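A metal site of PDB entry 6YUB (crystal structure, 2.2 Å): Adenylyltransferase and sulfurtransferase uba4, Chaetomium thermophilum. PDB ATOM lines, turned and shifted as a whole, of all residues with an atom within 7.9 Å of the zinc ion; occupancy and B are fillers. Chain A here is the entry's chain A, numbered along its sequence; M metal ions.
The backbone carbonyl oxygen of Cys 186 sits at hydrogen-bond distance from the side-chain amino group of Lys 275, at 3.0 Å. ND2 of Asn 311 lies close to O of Cys 186, at 3.5 Å. The side-chain sulfur of Cys 281 lies close to the guanidinium group of Arg 274. The side-chain sulfur (SG) of Cys 278 sits close to the backbone NH (N) of Ala 280 (3.4 Å). N of Arg 185 lies close to SG of Cys 183 (3.1 Å). The side-chain sulfur (SG) of Cys 187 is in hydrogen-bond range of the backbone carbonyl oxygen (O) of Cys 183 (3.7 Å).
Four residues have an atom within 4 Å of the zinc ion: Cys 183, Cys 186, Cys 278 and Cys 281. Along chain A the residues within 4 Å of the zinc ion span positions 183 to 281.
The zinc ion is bound by the side-chain sulfur (SG) of Cys 186, the side-chain sulfur (SG) of Cys 281, the side-chain sulfur (SG) of Cys 278 and the side-chain sulfur (SG) of Cys 183.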
ATOM      1  N   SER A 141     -25.932   5.576   0.287  1.00  0.00           N
ATOM      2  CA  SER A 141     -25.141   5.767  -0.920  1.00  0.00           C
ATOM      3  C   SER A 141     -24.611   4.440  -1.452  1.00  0.00           C
ATOM      4  O   SER A 141     -24.679   4.168  -2.654  1.00  0.00           O
ATOM      5  CB  SER A 141     -23.978   6.728  -0.632  1.00  0.00           C
ATOM      6  OG  SER A 141     -23.268   7.050  -1.816  1.00  0.00           O
ATOM      7  N   ASP A 142     -24.105   3.592  -0.552  1.00  0.00           N
ATOM      8  CA  ASP A 142     -23.618   2.275  -0.962  1.00  0.00           C
ATOM      9  C   ASP A 142     -24.718   1.486  -1.669  1.00  0.00           C
ATOM     10  O   ASP A 142     -24.500   0.928  -2.755  1.00  0.00           O
ATOM     11  CB  ASP A 142     -23.122   1.498   0.264  1.00  0.00           C
ATOM     12  CG  ASP A 142     -21.811   2.016   0.789  1.00  0.00           C
ATOM     13  OD1 ASP A 142     -21.220   2.931   0.157  1.00  0.00           O
ATOM     14  OD2 ASP A 142     -21.347   1.507   1.831  1.00  0.00           O
ATOM     15  N   VAL A 145     -25.624   2.894  -5.099  1.00  0.00           N
ATOM     16  CA  VAL A 145     -24.647   2.531  -6.108  1.00  0.00           C
ATOM     17  C   VAL A 145     -24.876   1.101  -6.583  1.00  0.00           C
ATOM     18  O   VAL A 145     -24.871   0.806  -7.776  1.00  0.00           O
ATOM     19  CB  VAL A 145     -23.215   2.725  -5.574  1.00  0.00           C
ATOM     20  CG1 VAL A 145     -22.211   1.993  -6.445  1.00  0.00           C
ATOM     21  CG2 VAL A 145     -22.880   4.204  -5.480  1.00  0.00           C
ATOM     22  N   ALA A 181     -20.909   9.865 -12.457  1.00  0.00           N
ATOM     23  CA  ALA A 181     -21.155  10.697 -11.289  1.00  0.00           C
ATOM     24  C   ALA A 181     -20.540  10.056 -10.049  1.00  0.00           C
ATOM     25  O   ALA A 181     -20.345   8.835  -9.995  1.00  0.00           O
ATOM     26  CB  ALA A 181     -22.648  10.913 -11.095  1.00  0.00           C
ATOM     27  N   PRO A 182     -20.227  10.857  -9.041  1.00  0.00           N
ATOM     28  CA  PRO A 182     -19.638  10.305  -7.813  1.00  0.00           C
ATOM     29  C   PRO A 182     -20.692   9.750  -6.867  1.00  0.00           C
ATOM     30  O   PRO A 182     -21.882  10.008  -6.998  1.00  0.00           O
ATOM     31  CB  PRO A 182     -18.927  11.508  -7.192  1.00  0.00           C
ATOM     32  CG  PRO A 182     -19.801  12.668  -7.595  1.00  0.00           C
ATOM     33  CD  PRO A 182     -20.378  12.325  -8.966  1.00  0.00           C
ATOM     34  N   CYS A 183     -20.224   8.953  -5.917  1.00  0.00           N
ATOM     35  CA  CYS A 183     -21.026   8.531  -4.773  1.00  0.00           C
ATOM     36  C   CYS A 183     -20.574   9.326  -3.556  1.00  0.00           C
ATOM     37  O   CYS A 183     -19.677  10.176  -3.628  1.00  0.00           O
ATOM     38  CB  CYS A 183     -20.918   7.022  -4.557  1.00  0.00           C
ATOM     39  SG  CYS A 183     -19.629   6.516  -3.411  1.00  0.00           S
ATOM     40  N   TYR A 184     -21.203   9.049  -2.415  1.00  0.00           N
ATOM     41  CA  TYR A 184     -20.879   9.833  -1.223  1.00  0.00           C
ATOM     42  C   TYR A 184     -19.478   9.526  -0.709  1.00  0.00           C
ATOM     43  O   TYR A 184     -18.855  10.390  -0.073  1.00  0.00           O
ATOM     44  CB  TYR A 184     -21.901   9.581  -0.118  1.00  0.00           C
ATOM     45  CG  TYR A 184     -21.870  10.645   0.963  1.00  0.00           C
ATOM     46  CD1 TYR A 184     -22.481  11.874   0.757  1.00  0.00           C
ATOM     47  CD2 TYR A 184     -21.238  10.412   2.173  1.00  0.00           C
ATOM     48  CE1 TYR A 184     -22.453  12.850   1.725  1.00  0.00           C
ATOM     49  CE2 TYR A 184     -21.215  11.386   3.155  1.00  0.00           C
ATOM     50  CZ  TYR A 184     -21.824  12.594   2.926  1.00  0.00           C
ATOM     51  OH  TYR A 184     -21.816  13.582   3.903  1.00  0.00           O
ATOM     52  N   ARG A 185     -18.962   8.326  -0.958  1.00  0.00           N
ATOM     53  CA  ARG A 185     -17.598   8.015  -0.563  1.00  0.00           C
ATOM     54  C   ARG A 185     -16.587   8.721  -1.470  1.00  0.00           C
ATOM     55  O   ARG A 185     -15.566   9.222  -0.991  1.00  0.00           O
ATOM     56  CB  ARG A 185     -17.365   6.506  -0.573  1.00  0.00           C
ATOM     57  CG  ARG A 185     -18.050   5.763   0.555  1.00  0.00           C
ATOM     58  CD  ARG A 185     -17.821   4.263   0.447  1.00  0.00           C
ATOM     59  NE  ARG A 185     -18.685   3.501   1.343  1.00  0.00           N
ATOM     60  CZ  ARG A 185     -18.409   3.264   2.620  1.00  0.00           C
ATOM     61  NH1 ARG A 185     -17.298   3.735   3.167  1.00  0.00           N
ATOM     62  NH2 ARG A 185     -19.263   2.567   3.358  1.00  0.00           N
ATOM     63  N   CYS A 186     -16.870   8.774  -2.769  1.00  0.00           N
ATOM     64  CA  CYS A 186     -16.021   9.544  -3.677  1.00  0.00           C
ATOM     65  C   CYS A 186     -15.855  10.983  -3.195  1.00  0.00           C
ATOM     66  O   CYS A 186     -14.789  11.574  -3.365  1.00  0.00           O
ATOM     67  CB  CYS A 186     -16.615   9.554  -5.084  1.00  0.00           C
ATOM     68  SG  CYS A 186     -16.559   7.978  -5.970  1.00  0.00           S
ATOM     69  N   CYS A 187     -16.891  11.535  -2.565  1.00  0.00           N
ATOM     70  CA  CYS A 187     -16.898  12.940  -2.155  1.00  0.00           C
ATOM     71  C   CYS A 187     -16.372  13.150  -0.744  1.00  0.00           C
ATOM     72  O   CYS A 187     -15.669  14.124  -0.494  1.00  0.00           O
ATOM     73  CB  CYS A 187     -18.314  13.504  -2.274  1.00  0.00           C
ATOM     74  SG  CYS A 187     -18.885  13.742  -3.982  1.00  0.00           S
ATOM     75  N   PHE A 188     -16.719  12.255   0.189  1.00  0.00           N
ATOM     76  CA  PHE A 188     -16.301  12.369   1.585  1.00  0.00           C
ATOM     77  C   PHE A 188     -15.787  11.014   2.049  1.00  0.00           C
ATOM     78  O   PHE A 188     -16.561  10.187   2.552  1.00  0.00           O
ATOM     79  CB  PHE A 188     -17.460  12.855   2.467  1.00  0.00           C
ATOM     80  CG  PHE A 188     -18.164  14.073   1.948  1.00  0.00           C
ATOM     81  CD1 PHE A 188     -19.230  13.953   1.069  1.00  0.00           C
ATOM     82  CD2 PHE A 188     -17.763  15.345   2.347  1.00  0.00           C
ATOM     83  CE1 PHE A 188     -19.881  15.075   0.593  1.00  0.00           C
ATOM     84  CE2 PHE A 188     -18.401  16.467   1.869  1.00  0.00           C
ATOM     85  CZ  PHE A 188     -19.468  16.330   0.989  1.00  0.00           C
ATOM     86  N   GLY A 273     -15.868  13.795 -10.532  1.00  0.00           N
ATOM     87  CA  GLY A 273     -16.669  12.638 -10.866  1.00  0.00           C
ATOM     88  C   GLY A 273     -16.305  11.459  -9.979  1.00  0.00           C
ATOM     89  O   GLY A 273     -15.692  11.579  -8.933  1.00  0.00           O
ATOM     90  N   ARG A 274     -16.722  10.269 -10.446  1.00  0.00           N
ATOM     91  CA  ARG A 274     -16.407   9.038  -9.730  1.00  0.00           C
ATOM     92  C   ARG A 274     -14.902   8.856  -9.593  1.00  0.00           C
ATOM     93  O   ARG A 274     -14.142   9.055 -10.540  1.00  0.00           O
ATOM     94  CB  ARG A 274     -17.016   7.833 -10.465  1.00  0.00           C
ATOM     95  CG  ARG A 274     -16.488   6.480 -10.041  1.00  0.00           C
ATOM     96  CD  ARG A 274     -17.252   5.359 -10.744  1.00  0.00           C
ATOM     97  NE  ARG A 274     -18.612   5.235 -10.230  1.00  0.00           N
ATOM     98  CZ  ARG A 274     -19.554   4.474 -10.787  1.00  0.00           C
ATOM     99  NH1 ARG A 274     -19.288   3.779 -11.887  1.00  0.00           N
ATOM    100  NH2 ARG A 274     -20.762   4.418 -10.251  1.00  0.00           N
ATOM    101  N   LYS A 275     -14.466   8.480  -8.387  1.00  0.00           N
ATOM    102  CA  LYS A 275     -13.059   8.175  -8.157  1.00  0.00           C
ATOM    103  C   LYS A 275     -12.767   6.732  -8.571  1.00  0.00           C
ATOM    104  O   LYS A 275     -13.518   5.817  -8.269  1.00  0.00           O
ATOM    105  CB  LYS A 275     -12.708   8.367  -6.675  1.00  0.00           C
ATOM    106  CG  LYS A 275     -12.614   9.803  -6.234  1.00  0.00           C
ATOM    107  CD  LYS A 275     -12.249   9.898  -4.768  1.00  0.00           C
ATOM    108  CE  LYS A 275     -11.690  11.276  -4.440  1.00  0.00           C
ATOM    109  NZ  LYS A 275     -11.781  11.583  -2.977  1.00  0.00           N
ATOM    110  N   LYS A 276     -11.646   6.553  -9.282  1.00  0.00           N
ATOM    111  CA  LYS A 276     -11.297   5.224  -9.774  1.00  0.00           C
ATOM    112  C   LYS A 276     -11.049   4.251  -8.628  1.00  0.00           C
ATOM    113  O   LYS A 276     -11.205   3.035  -8.807  1.00  0.00           O
ATOM    114  CB  LYS A 276     -10.067   5.316 -10.677  1.00  0.00           C
ATOM    115  CG  LYS A 276     -10.204   4.559 -11.995  1.00  0.00           C
ATOM    116  CD  LYS A 276      -9.525   5.326 -13.125  1.00  0.00           C
ATOM    117  N   ASP A 277     -10.651   4.753  -7.465  1.00  0.00           N
ATOM    118  CA  ASP A 277     -10.282   3.912  -6.327  1.00  0.00           C
ATOM    119  C   ASP A 277     -11.322   3.951  -5.211  1.00  0.00           C
ATOM    120  O   ASP A 277     -11.001   3.628  -4.059  1.00  0.00           O
ATOM    121  CB  ASP A 277      -8.922   4.337  -5.782  1.00  0.00           C
ATOM    122  CG  ASP A 277      -8.951   5.726  -5.171  1.00  0.00           C
ATOM    123  OD1 ASP A 277      -9.824   6.530  -5.544  1.00  0.00           O
ATOM    124  OD2 ASP A 277      -8.082   6.019  -4.315  1.00  0.00           O
ATOM    125  N   CYS A 278     -12.560   4.327  -5.518  1.00  0.00           N
ATOM    126  CA  CYS A 278     -13.575   4.440  -4.486  1.00  0.00           C
ATOM    127  C   CYS A 278     -13.913   3.065  -3.912  1.00  0.00           C
ATOM    128  O   CYS A 278     -14.084   2.090  -4.638  1.00  0.00           O
ATOM    129  CB  CYS A 278     -14.852   5.068  -5.048  1.00  0.00           C
ATOM    130  SG  CYS A 278     -16.197   5.167  -3.843  1.00  0.00           S
ATOM    131  N   PHE A 279     -14.005   3.006  -2.577  1.00  0.00           N
ATOM    132  CA  PHE A 279     -14.289   1.740  -1.900  1.00  0.00           C
ATOM    133  C   PHE A 279     -15.601   1.136  -2.364  1.00  0.00           C
ATOM    134  O   PHE A 279     -15.734  -0.100  -2.407  1.00  0.00           O
ATOM    135  CB  PHE A 279     -14.318   1.980  -0.388  1.00  0.00           C
ATOM    136  CG  PHE A 279     -14.870   0.827   0.409  1.00  0.00           C
ATOM    137  CD1 PHE A 279     -14.067  -0.262   0.716  1.00  0.00           C
ATOM    138  CD2 PHE A 279     -16.181   0.835   0.837  1.00  0.00           C
ATOM    139  CE1 PHE A 279     -14.575  -1.325   1.452  1.00  0.00           C
ATOM    140  CE2 PHE A 279     -16.697  -0.227   1.562  1.00  0.00           C
ATOM    141  CZ  PHE A 279     -15.886  -1.305   1.872  1.00  0.00           C
ATOM    142  N   ALA A 280     -16.581   1.959  -2.737  1.00  0.00           N
ATOM    143  CA  ALA A 280     -17.912   1.472  -3.064  1.00  0.00           C
ATOM    144  C   ALA A 280     -18.163   1.367  -4.572  1.00  0.00           C
ATOM    145  O   ALA A 280     -18.684   0.353  -5.037  1.00  0.00           O
ATOM    146  CB  ALA A 280     -18.970   2.385  -2.427  1.00  0.00           C
ATOM    147  N   CYS A 281     -17.814   2.398  -5.337  1.00  0.00           N
ATOM    148  CA  CYS A 281     -18.128   2.436  -6.761  1.00  0.00           C
ATOM    149  C   CYS A 281     -16.911   2.284  -7.662  1.00  0.00           C
ATOM    150  O   CYS A 281     -17.082   2.179  -8.892  1.00  0.00           O
ATOM    151  CB  CYS A 281     -18.846   3.743  -7.107  1.00  0.00           C
ATOM    152  SG  CYS A 281     -17.855   5.241  -6.893  1.00  0.00           S
ATOM    153  N   GLY A 282     -15.696   2.272  -7.114  1.00  0.00           N
ATOM    154  CA  GLY A 282     -14.503   2.172  -7.922  1.00  0.00           C
ATOM    155  C   GLY A 282     -14.252   0.763  -8.417  1.00  0.00           C
ATOM    156  O   GLY A 282     -14.984  -0.181  -8.125  1.00  0.00           O
ATOM    157  N   ASN A 311     -12.885  15.658  -2.904  1.00  0.00           N
ATOM    158  CA  ASN A 311     -12.715  15.687  -4.356  1.00  0.00           C
ATOM    159  C   ASN A 311     -13.334  16.962  -4.939  1.00  0.00           C
ATOM    160  O   ASN A 311     -14.055  16.955  -5.933  1.00  0.00           O
ATOM    161  CB  ASN A 311     -13.296  14.437  -5.001  1.00  0.00           C
ATOM    162  CG  ASN A 311     -14.815  14.453  -5.086  1.00  0.00           C
ATOM    163  OD1 ASN A 311     -15.494  15.142  -4.317  1.00  0.00           O
ATOM    164  ND2 ASN A 311     -15.360  13.704  -6.040  1.00  0.00           N
HETATM  165 ZN    ZN M   1     -17.819   6.408  -4.944  1.00  0.00          ZN
